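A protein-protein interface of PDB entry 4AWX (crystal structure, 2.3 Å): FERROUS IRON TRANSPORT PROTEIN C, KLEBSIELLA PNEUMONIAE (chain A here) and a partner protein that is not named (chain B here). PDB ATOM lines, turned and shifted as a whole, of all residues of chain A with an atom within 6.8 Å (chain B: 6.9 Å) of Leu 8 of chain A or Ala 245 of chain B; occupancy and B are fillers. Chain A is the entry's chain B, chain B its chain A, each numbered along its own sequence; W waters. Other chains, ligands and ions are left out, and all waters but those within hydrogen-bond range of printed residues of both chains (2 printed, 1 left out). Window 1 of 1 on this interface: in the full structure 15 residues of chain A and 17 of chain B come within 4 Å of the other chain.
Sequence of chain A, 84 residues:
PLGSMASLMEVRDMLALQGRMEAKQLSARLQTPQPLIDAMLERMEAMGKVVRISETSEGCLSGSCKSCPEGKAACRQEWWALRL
The side-chain hydroxyl (OG) of Ser 7 of chain A lies within hydrogen-bond range of the side-chain carboxylate (OD1) of Asp 246 of chain B.
The backbone NH of Leu 8 of chain A is in hydrogen-bond range of the side-chain carboxylate of Asp 246 of chain B, at 2.6 Å.
O of Ala 6 of chain A lies close to OE1 of Gln 250 of chain B.
OH of Tyr 103 of chain B lies within hydrogen-bond range of OE2 of Glu 210 of chain B (2.8 Å).
NH1 of Arg 248 of chain B lies within hydrogen-bond range of OH of Tyr 103 of chain B.
N of Met 9 of chain A sits close to OG of Ser 7 of chain A, at 3.3 Å.
The backbone NH (N) of Ser 7 of chain A sits close to the side-chain carboxylate (OE1) of Glu 10 of chain A.
The side-chain carboxylate (OD1) of Asp 13 of chain A is in salt-bridge range of the guanidinium group (NH2) of Arg 12 of chain A, 3.2 Å away.
Among the printed residues, pairs that only touch across the chains: Met 9 of chain A with His 243 of chain B, Met 47 of chain A with Ala 241 of chain B, Ala 39 of chain A with Tyr 249 of chain B, Met 9 of chain A with Asp 246 of chain B, Leu 8 of chain A with Ala 245 of chain B, Arg 12 of chain A with Leu 242 of chain B, Arg 43 of chain A with Tyr 103 of chain B, Arg 43 of chain A with Tyr 249 of chain B, Met 47 of chain A with Ala 245 of chain B, Met 9 of chain A with Leu 242 of chain B and Leu 8 of chain A with Leu 242 of chain B.
Of the printed residues of chain B, Ser 7 of chain A touches Asp 246.
Leu 8 of chain A touches three residues of chain B.
Of the printed residues of chain B, Met 9 of chain A touches Leu 242, His 243 and Asp 246.
Of the printed residues of chain B, Ala 39 of chain A touches Tyr 249 (3.5 Å).
Of the printed residues of chain B, Arg 43 of chain A touches Tyr 103 (3.7 Å) and Tyr 249 (3.8 Å).
Ala 245 of chain B touches two residues of chain A.
The nearest printed residue of chain A that does not touch Tyr 103 of chain B is Met 47 of chain A (5.7 Å).
Hydrophobic or aromatic side chains of chain A that line the printed part of chain B: Leu 8, Met 9, Ala 39 and Met 47.
Hydrophobic or aromatic side chains of chain B within 4 Å of the printed part of chain A: Tyr 103, Ala 241, Leu 242, His 243, Ala 245 and Tyr 249.
Among the printed residues, 14 pairs touch across the chains.
Among the printed residues, no Asp or Glu carboxylate lies within 4 Å of a Lys or Arg side-chain nitrogen of the other chain.
Water W1 lies within hydrogen-bond range of the side-chain carboxylate of Glu 210 of chain B, the guanidinium group of Arg 43 of chain A, the side-chain hydroxyl of Tyr 103 of chain B and the side-chain sulfur of Met 47 of chain A.
Water W2 lies within hydrogen-bond range of the backbone carbonyl oxygen (O) of Gln 250 of chain B and the side-chain sulfur (SD) of Met 5 of chain A.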
ATOM      1  N   MET A   5      13.250 -12.147  22.860  1.00  0.00           N
ATOM      2  CA  MET A   5      12.598 -10.984  22.390  1.00  0.00           C
ATOM      3  C   MET A   5      11.120 -10.980  22.037  1.00  0.00           C
ATOM      4  O   MET A   5      10.350 -11.889  22.400  1.00  0.00           O
ATOM      5  CB  MET A   5      13.452 -10.432  21.260  1.00  0.00           C
ATOM      6  CG  MET A   5      13.739 -11.461  20.157  1.00  0.00           C
ATOM      7  SD  MET A   5      15.418 -11.321  19.378  1.00  0.00           S
ATOM      8  CE  MET A   5      16.086  -9.847  20.239  1.00  0.00           C
ATOM      9  N   ALA A   6      10.724  -9.944  21.325  1.00  0.00           N
ATOM     10  CA  ALA A   6       9.341  -9.753  21.007  1.00  0.00           C
ATOM     11  C   ALA A   6       8.547 -10.994  20.620  1.00  0.00           C
ATOM     12  O   ALA A   6       8.925 -11.773  19.733  1.00  0.00           O
ATOM     13  CB  ALA A   6       9.193  -8.632  19.937  1.00  0.00           C
ATOM     14  N   SER A   7       7.476 -11.303  21.322  1.00  0.00           N
ATOM     15  CA  SER A   7       6.751 -12.450  20.866  1.00  0.00           C
ATOM     16  C   SER A   7       5.433 -11.881  20.363  1.00  0.00           C
ATOM     17  O   SER A   7       4.927 -10.921  20.942  1.00  0.00           O
ATOM     18  CB  SER A   7       6.548 -13.468  21.993  1.00  0.00           C
ATOM     19  OG  SER A   7       5.805 -14.578  21.528  1.00  0.00           O
ATOM     20  N   LEU A   8       4.903 -12.399  19.256  1.00  0.00           N
ATOM     21  CA  LEU A   8       3.626 -11.888  18.798  1.00  0.00           C
ATOM     22  C   LEU A   8       2.693 -12.038  19.986  1.00  0.00           C
ATOM     23  O   LEU A   8       1.777 -11.232  20.175  1.00  0.00           O
ATOM     24  CB  LEU A   8       3.068 -12.690  17.619  1.00  0.00           C
ATOM     25  CG  LEU A   8       3.561 -12.402  16.200  1.00  0.00           C
ATOM     26  CD1 LEU A   8       2.629 -13.073  15.205  1.00  0.00           C
ATOM     27  CD2 LEU A   8       3.578 -10.909  15.935  1.00  0.00           C
ATOM     28  N   MET A   9       2.919 -13.077  20.785  1.00  0.00           N
ATOM     29  CA  MET A   9       2.085 -13.295  21.960  1.00  0.00           C
ATOM     30  C   MET A   9       2.281 -12.133  22.926  1.00  0.00           C
ATOM     31  O   MET A   9       1.318 -11.609  23.495  1.00  0.00           O
ATOM     32  CB  MET A   9       2.438 -14.609  22.664  1.00  0.00           C
ATOM     33  CG  MET A   9       1.671 -15.799  22.143  1.00  0.00           C
ATOM     34  SD  MET A   9       2.232 -16.281  20.518  1.00  0.00           S
ATOM     35  CE  MET A   9       3.739 -17.203  20.942  1.00  0.00           C
ATOM     36  N   GLU A  10       3.540 -11.747  23.102  1.00  0.00           N
ATOM     37  CA  GLU A  10       3.891 -10.647  23.983  1.00  0.00           C
ATOM     38  C   GLU A  10       3.117  -9.395  23.556  1.00  0.00           C
ATOM     39  O   GLU A  10       2.546  -8.697  24.395  1.00  0.00           O
ATOM     40  CB  GLU A  10       5.395 -10.379  23.907  1.00  0.00           C
ATOM     41  CG  GLU A  10       6.160 -10.579  25.227  1.00  0.00           C
ATOM     42  CD  GLU A  10       6.999 -11.858  25.256  1.00  0.00           C
ATOM     43  OE1 GLU A  10       7.906 -12.004  24.395  1.00  0.00           O
ATOM     44  OE2 GLU A  10       6.749 -12.709  26.148  1.00  0.00           O
ATOM     45  N   VAL A  11       3.103  -9.118  22.256  1.00  0.00           N
ATOM     46  CA  VAL A  11       2.389  -7.961  21.726  1.00  0.00           C
ATOM     47  C   VAL A  11       0.903  -8.112  22.080  1.00  0.00           C
ATOM     48  O   VAL A  11       0.268  -7.171  22.561  1.00  0.00           O
ATOM     49  CB  VAL A  11       2.565  -7.842  20.186  1.00  0.00           C
ATOM     50  CG1 VAL A  11       1.697  -6.728  19.633  1.00  0.00           C
ATOM     51  CG2 VAL A  11       4.011  -7.552  19.854  1.00  0.00           C
ATOM     52  N   ARG A  12       0.358  -9.309  21.866  1.00  0.00           N
ATOM     53  CA  ARG A  12      -1.046  -9.570  22.176  1.00  0.00           C
ATOM     54  C   ARG A  12      -1.341  -9.292  23.643  1.00  0.00           C
ATOM     55  O   ARG A  12      -2.229  -8.494  23.967  1.00  0.00           O
ATOM     56  CB  ARG A  12      -1.411 -11.022  21.886  1.00  0.00           C
ATOM     57  CG  ARG A  12      -2.835 -11.374  22.294  1.00  0.00           C
ATOM     58  CD  ARG A  12      -3.035 -12.875  22.375  1.00  0.00           C
ATOM     59  NE  ARG A  12      -2.167 -13.484  23.378  1.00  0.00           N
ATOM     60  CZ  ARG A  12      -2.029 -14.797  23.555  1.00  0.00           C
ATOM     61  NH1 ARG A  12      -2.698 -15.660  22.792  1.00  0.00           N
ATOM     62  NH2 ARG A  12      -1.212 -15.257  24.496  1.00  0.00           N
ATOM     63  N   ASP A  13      -0.599  -9.972  24.519  1.00  0.00           N
ATOM     64  CA  ASP A  13      -0.756  -9.828  25.963  1.00  0.00           C
ATOM     65  C   ASP A  13      -0.698  -8.369  26.376  1.00  0.00           C
ATOM     66  O   ASP A  13      -1.580  -7.880  27.087  1.00  0.00           O
ATOM     67  CB  ASP A  13       0.331 -10.615  26.703  1.00  0.00           C
ATOM     68  CG  ASP A  13       0.165 -12.126  26.562  1.00  0.00           C
ATOM     69  OD1 ASP A  13      -0.967 -12.584  26.290  1.00  0.00           O
ATOM     70  OD2 ASP A  13       1.169 -12.855  26.743  1.00  0.00           O
ATOM     71  N   LEU A  36      10.250  -3.941  13.229  1.00  0.00           N
ATOM     72  CA  LEU A  36       9.852  -5.287  13.611  1.00  0.00           C
ATOM     73  C   LEU A  36       8.433  -5.202  14.166  1.00  0.00           C
ATOM     74  O   LEU A  36       7.567  -6.011  13.834  1.00  0.00           O
ATOM     75  CB  LEU A  36      10.793  -5.848  14.685  1.00  0.00           C
ATOM     76  CG  LEU A  36      11.505  -7.172  14.370  1.00  0.00           C
ATOM     77  CD1 LEU A  36      12.299  -7.642  15.576  1.00  0.00           C
ATOM     78  CD2 LEU A  36      10.482  -8.223  13.988  1.00  0.00           C
ATOM     79  N   ALA A  39       5.767  -4.523  11.425  1.00  0.00           N
ATOM     80  CA  ALA A  39       5.505  -5.731  10.652  1.00  0.00           C
ATOM     81  C   ALA A  39       4.691  -6.759  11.436  1.00  0.00           C
ATOM     82  O   ALA A  39       3.839  -7.444  10.877  1.00  0.00           O
ATOM     83  CB  ALA A  39       6.817  -6.350  10.187  1.00  0.00           C
ATOM     84  N   MET A  40       4.961  -6.864  12.733  1.00  0.00           N
ATOM     85  CA  MET A  40       4.242  -7.805  13.579  1.00  0.00           C
ATOM     86  C   MET A  40       2.774  -7.400  13.706  1.00  0.00           C
ATOM     87  O   MET A  40       1.889  -8.251  13.662  1.00  0.00           O
ATOM     88  CB  MET A  40       4.905  -7.888  14.958  1.00  0.00           C
ATOM     89  CG  MET A  40       6.233  -8.646  14.943  1.00  0.00           C
ATOM     90  SD  MET A  40       7.195  -8.565  16.482  1.00  0.00           S
ATOM     91  CE  MET A  40       6.406  -9.905  17.471  1.00  0.00           C
ATOM     92  N   LEU A  41       2.519  -6.100  13.856  1.00  0.00           N
ATOM     93  CA  LEU A  41       1.151  -5.598  13.967  1.00  0.00           C
ATOM     94  C   LEU A  41       0.360  -5.904  12.702  1.00  0.00           C
ATOM     95  O   LEU A  41      -0.745  -6.447  12.765  1.00  0.00           O
ATOM     96  CB  LEU A  41       1.142  -4.082  14.210  1.00  0.00           C
ATOM     97  CG  LEU A  41       1.039  -3.490  15.620  1.00  0.00           C
ATOM     98  CD1 LEU A  41       1.031  -4.579  16.671  1.00  0.00           C
ATOM     99  CD2 LEU A  41       2.190  -2.528  15.831  1.00  0.00           C
ATOM    100  N   ARG A  43       0.838  -8.159  10.511  1.00  0.00           N
ATOM    101  CA  ARG A  43       0.621  -9.594  10.401  1.00  0.00           C
ATOM    102  C   ARG A  43      -0.576 -10.005  11.255  1.00  0.00           C
ATOM    103  O   ARG A  43      -1.471 -10.719  10.792  1.00  0.00           O
ATOM    104  CB  ARG A  43       1.869 -10.354  10.866  1.00  0.00           C
ATOM    105  CG  ARG A  43       1.923 -11.779  10.387  1.00  0.00           C
ATOM    106  CD  ARG A  43       1.935 -11.785   8.873  1.00  0.00           C
ATOM    107  NE  ARG A  43       0.914 -12.674   8.360  1.00  0.00           N
ATOM    108  CZ  ARG A  43       0.248 -12.484   7.228  1.00  0.00           C
ATOM    109  NH1 ARG A  43       0.487 -11.421   6.473  1.00  0.00           N
ATOM    110  NH2 ARG A  43      -0.666 -13.369   6.867  1.00  0.00           N
ATOM    111  N   MET A  44      -0.581  -9.556  12.505  1.00  0.00           N
ATOM    112  CA  MET A  44      -1.677  -9.870  13.412  1.00  0.00           C
ATOM    113  C   MET A  44      -2.969  -9.255  12.877  1.00  0.00           C
ATOM    114  O   MET A  44      -4.051  -9.811  13.056  1.00  0.00           O
ATOM    115  CB  MET A  44      -1.376  -9.340  14.821  1.00  0.00           C
ATOM    116  CG  MET A  44      -0.139  -9.951  15.475  1.00  0.00           C
ATOM    117  SD  MET A  44       0.267  -9.185  17.074  1.00  0.00           S
ATOM    118  CE  MET A  44      -0.906 -10.021  18.137  1.00  0.00           C
ATOM    119  N   MET A  47      -4.367 -11.333  10.177  1.00  0.00           N
ATOM    120  CA  MET A  47      -4.938 -12.531  10.772  1.00  0.00           C
ATOM    121  C   MET A  47      -6.275 -12.207  11.448  1.00  0.00           C
ATOM    122  O   MET A  47      -7.064 -13.100  11.757  1.00  0.00           O
ATOM    123  CB  MET A  47      -3.954 -13.143  11.772  1.00  0.00           C
ATOM    124  CG  MET A  47      -2.663 -13.644  11.133  1.00  0.00           C
ATOM    125  SD  MET A  47      -1.501 -14.331  12.346  1.00  0.00           S
ATOM    126  CE  MET A  47      -2.178 -15.925  12.590  1.00  0.00           C
ATOM    127  N   TYR B 103       8.451 -12.652   5.496  1.00  0.00           N
ATOM    128  CA  TYR B 103       7.431 -13.587   5.916  1.00  0.00           C
ATOM    129  C   TYR B 103       7.083 -14.498   4.729  1.00  0.00           C
ATOM    130  O   TYR B 103       6.997 -15.709   4.885  1.00  0.00           O
ATOM    131  CB  TYR B 103       6.173 -12.865   6.396  1.00  0.00           C
ATOM    132  CG  TYR B 103       5.226 -13.788   7.123  1.00  0.00           C
ATOM    133  CD1 TYR B 103       5.421 -14.094   8.469  1.00  0.00           C
ATOM    134  CD2 TYR B 103       4.158 -14.389   6.459  1.00  0.00           C
ATOM    135  CE1 TYR B 103       4.578 -14.971   9.138  1.00  0.00           C
ATOM    136  CE2 TYR B 103       3.306 -15.273   7.118  1.00  0.00           C
ATOM    137  CZ  TYR B 103       3.520 -15.559   8.460  1.00  0.00           C
ATOM    138  OH  TYR B 103       2.674 -16.415   9.127  1.00  0.00           O
ATOM    139  N   TYR B 177       9.286 -24.145  15.891  1.00  0.00           N
ATOM    140  CA  TYR B 177       7.896 -24.153  16.324  1.00  0.00           C
ATOM    141  C   TYR B 177       7.742 -24.962  17.603  1.00  0.00           C
ATOM    142  O   TYR B 177       8.542 -25.855  17.877  1.00  0.00           O
ATOM    143  CB  TYR B 177       7.008 -24.800  15.259  1.00  0.00           C
ATOM    144  CG  TYR B 177       6.966 -24.091  13.929  1.00  0.00           C
ATOM    145  CD1 TYR B 177       6.134 -22.986  13.731  1.00  0.00           C
ATOM    146  CD2 TYR B 177       7.753 -24.526  12.861  1.00  0.00           C
ATOM    147  CE1 TYR B 177       6.082 -22.335  12.509  1.00  0.00           C
ATOM    148  CE2 TYR B 177       7.708 -23.881  11.632  1.00  0.00           C
ATOM    149  CZ  TYR B 177       6.868 -22.779  11.464  1.00  0.00           C
ATOM    150  OH  TYR B 177       6.832 -22.095  10.275  1.00  0.00           O
ATOM    151  N   GLU B 210      -2.410 -22.609  11.155  1.00  0.00           N
ATOM    152  CA  GLU B 210      -2.233 -21.165  11.074  1.00  0.00           C
ATOM    153  C   GLU B 210      -3.516 -20.470  10.639  1.00  0.00           C
ATOM    154  O   GLU B 210      -3.643 -19.252  10.777  1.00  0.00           O
ATOM    155  CB  GLU B 210      -1.118 -20.818  10.082  1.00  0.00           C
ATOM    156  CG  GLU B 210      -0.819 -19.323   9.973  1.00  0.00           C
ATOM    157  CD  GLU B 210       0.250 -19.022   8.940  1.00  0.00           C
ATOM    158  OE1 GLU B 210       1.032 -19.942   8.618  1.00  0.00           O
ATOM    159  OE2 GLU B 210       0.321 -17.868   8.454  1.00  0.00           O
ATOM    160  N   PRO B 240      -3.012 -21.480  18.518  1.00  0.00           N
ATOM    161  CA  PRO B 240      -2.121 -22.150  17.573  1.00  0.00           C
ATOM    162  C   PRO B 240      -1.590 -21.238  16.462  1.00  0.00           C
ATOM    163  O   PRO B 240      -0.383 -21.119  16.277  1.00  0.00           O
ATOM    164  CB  PRO B 240      -3.001 -23.270  17.040  1.00  0.00           C
ATOM    165  CG  PRO B 240      -3.798 -23.645  18.249  1.00  0.00           C
ATOM    166  CD  PRO B 240      -4.189 -22.314  18.821  1.00  0.00           C
ATOM    167  N   ALA B 241      -2.503 -20.600  15.740  1.00  0.00           N
ATOM    168  CA  ALA B 241      -2.143 -19.725  14.634  1.00  0.00           C
ATOM    169  C   ALA B 241      -1.184 -18.605  15.012  1.00  0.00           C
ATOM    170  O   ALA B 241      -0.245 -18.309  14.267  1.00  0.00           O
ATOM    171  CB  ALA B 241      -3.385 -19.145  14.016  1.00  0.00           C
ATOM    172  N   LEU B 242      -1.419 -17.979  16.161  1.00  0.00           N
ATOM    173  CA  LEU B 242      -0.568 -16.900  16.610  1.00  0.00           C
ATOM    174  C   LEU B 242       0.823 -17.434  16.906  1.00  0.00           C
ATOM    175  O   LEU B 242       1.815 -16.736  16.737  1.00  0.00           O
ATOM    176  CB  LEU B 242      -1.132 -16.253  17.868  1.00  0.00           C
ATOM    177  CG  LEU B 242      -1.599 -14.798  17.842  1.00  0.00           C
ATOM    178  CD1 LEU B 242      -1.524 -14.259  19.273  1.00  0.00           C
ATOM    179  CD2 LEU B 242      -0.723 -13.952  16.944  1.00  0.00           C
ATOM    180  N   HIS B 243       0.901 -18.678  17.347  1.00  0.00           N
ATOM    181  CA  HIS B 243       2.187 -19.273  17.654  1.00  0.00           C
ATOM    182  C   HIS B 243       3.012 -19.569  16.402  1.00  0.00           C
ATOM    183  O   HIS B 243       4.228 -19.403  16.396  1.00  0.00           O
ATOM    184  CB  HIS B 243       1.989 -20.545  18.487  1.00  0.00           C
ATOM    185  CG  HIS B 243       1.687 -20.275  19.928  1.00  0.00           C
ATOM    186  ND1 HIS B 243       0.484 -19.755  20.356  1.00  0.00           N
ATOM    187  CD2 HIS B 243       2.458 -20.394  21.033  1.00  0.00           C
ATOM    188  CE1 HIS B 243       0.527 -19.560  21.661  1.00  0.00           C
ATOM    189  NE2 HIS B 243       1.714 -19.943  22.096  1.00  0.00           N
ATOM    190  N   ILE B 244       2.349 -20.005  15.341  1.00  0.00           N
ATOM    191  CA  ILE B 244       3.039 -20.308  14.100  1.00  0.00           C
ATOM    192  C   ILE B 244       3.590 -19.031  13.461  1.00  0.00           C
ATOM    193  O   ILE B 244       4.738 -19.008  13.021  1.00  0.00           O
ATOM    194  CB  ILE B 244       2.095 -21.052  13.136  1.00  0.00           C
ATOM    195  CG1 ILE B 244       1.769 -22.422  13.735  1.00  0.00           C
ATOM    196  CG2 ILE B 244       2.736 -21.205  11.775  1.00  0.00           C
ATOM    197  CD1 ILE B 244       0.756 -23.227  12.981  1.00  0.00           C
ATOM    198  N   ALA B 245       2.782 -17.972  13.439  1.00  0.00           N
ATOM    199  CA  ALA B 245       3.202 -16.700  12.865  1.00  0.00           C
ATOM    200  C   ALA B 245       4.317 -16.109  13.721  1.00  0.00           C
ATOM    201  O   ALA B 245       5.304 -15.576  13.204  1.00  0.00           O
ATOM    202  CB  ALA B 245       2.015 -15.731  12.785  1.00  0.00           C
ATOM    203  N   ASP B 246       4.153 -16.214  15.037  1.00  0.00           N
ATOM    204  CA  ASP B 246       5.147 -15.724  15.977  1.00  0.00           C
ATOM    205  C   ASP B 246       6.478 -16.443  15.789  1.00  0.00           C
ATOM    206  O   ASP B 246       7.538 -15.817  15.822  1.00  0.00           O
ATOM    207  CB  ASP B 246       4.702 -15.945  17.420  1.00  0.00           C
ATOM    208  CG  ASP B 246       5.862 -15.790  18.410  1.00  0.00           C
ATOM    209  OD1 ASP B 246       6.160 -14.640  18.808  1.00  0.00           O
ATOM    210  OD2 ASP B 246       6.496 -16.812  18.772  1.00  0.00           O
ATOM    211  N   ALA B 247       6.425 -17.763  15.631  1.00  0.00           N
ATOM    212  CA  ALA B 247       7.639 -18.550  15.452  1.00  0.00           C
ATOM    213  C   ALA B 247       8.401 -18.047  14.238  1.00  0.00           C
ATOM    214  O   ALA B 247       9.611 -17.894  14.289  1.00  0.00           O
ATOM    215  CB  ALA B 247       7.300 -20.024  15.290  1.00  0.00           C
ATOM    216  N   ARG B 248       7.684 -17.789  13.147  1.00  0.00           N
ATOM    217  CA  ARG B 248       8.309 -17.290  11.925  1.00  0.00           C
ATOM    218  C   ARG B 248       8.915 -15.897  12.118  1.00  0.00           C
ATOM    219  O   ARG B 248       9.997 -15.615  11.609  1.00  0.00           O
ATOM    220  CB  ARG B 248       7.300 -17.265  10.778  1.00  0.00           C
ATOM    221  CG  ARG B 248       7.501 -18.380   9.797  1.00  0.00           C
ATOM    222  CD  ARG B 248       6.380 -18.422   8.788  1.00  0.00           C
ATOM    223  NE  ARG B 248       5.752 -19.736   8.758  1.00  0.00           N
ATOM    224  CZ  ARG B 248       4.469 -19.941   8.496  1.00  0.00           C
ATOM    225  NH1 ARG B 248       3.677 -18.915   8.243  1.00  0.00           N
ATOM    226  NH2 ARG B 248       3.976 -21.168   8.492  1.00  0.00           N
ATOM    227  N   TYR B 249       8.221 -15.024  12.842  1.00  0.00           N
ATOM    228  CA  TYR B 249       8.773 -13.703  13.082  1.00  0.00           C
ATOM    229  C   TYR B 249       9.994 -13.746  14.005  1.00  0.00           C
ATOM    230  O   TYR B 249      10.787 -12.812  14.031  1.00  0.00           O
ATOM    231  CB  TYR B 249       7.702 -12.736  13.604  1.00  0.00           C
ATOM    232  CG  TYR B 249       7.220 -11.845  12.480  1.00  0.00           C
ATOM    233  CD1 TYR B 249       8.046 -10.837  11.987  1.00  0.00           C
ATOM    234  CD2 TYR B 249       6.016 -12.095  11.811  1.00  0.00           C
ATOM    235  CE1 TYR B 249       7.705 -10.115  10.867  1.00  0.00           C
ATOM    236  CE2 TYR B 249       5.666 -11.369  10.682  1.00  0.00           C
ATOM    237  CZ  TYR B 249       6.520 -10.380  10.214  1.00  0.00           C
ATOM    238  OH  TYR B 249       6.222  -9.650   9.088  1.00  0.00           O
ATOM    239  N   GLN B 250      10.154 -14.843  14.741  1.00  0.00           N
ATOM    240  CA  GLN B 250      11.317 -15.002  15.610  1.00  0.00           C
ATOM    241  C   GLN B 250      12.554 -15.110  14.734  1.00  0.00           C
ATOM    242  O   GLN B 250      13.546 -14.432  14.972  1.00  0.00           O
ATOM    243  CB  GLN B 250      11.224 -16.274  16.457  1.00  0.00           C
ATOM    244  CG  GLN B 250      10.062 -16.314  17.413  1.00  0.00           C
ATOM    245  CD  GLN B 250      10.295 -15.460  18.630  1.00  0.00           C
ATOM    246  OE1 GLN B 250      10.858 -14.358  18.536  1.00  0.00           O
ATOM    247  NE2 GLN B 250       9.851 -15.955  19.796  1.00  0.00           N
ATOM    248  N   ILE B 252      12.749 -14.214  11.594  1.00  0.00           N
ATOM    249  CA  ILE B 252      12.850 -13.015  10.753  1.00  0.00           C
ATOM    250  C   ILE B 252      13.676 -11.998  11.537  1.00  0.00           C
ATOM    251  O   ILE B 252      14.561 -11.334  10.990  1.00  0.00           O
ATOM    252  CB  ILE B 252      11.469 -12.378  10.450  1.00  0.00           C
ATOM    253  CG1 ILE B 252      10.695 -13.248   9.463  1.00  0.00           C
ATOM    254  CG2 ILE B 252      11.652 -10.962   9.897  1.00  0.00           C
ATOM    255  CD1 ILE B 252       9.308 -12.718   9.161  1.00  0.00           C
HETATM  256  O   HOH W   1      -0.294 -15.483   8.941  1.00  0.00           O
HETATM  257  O   HOH W   2      15.077 -13.793  17.476  1.00  0.00           O
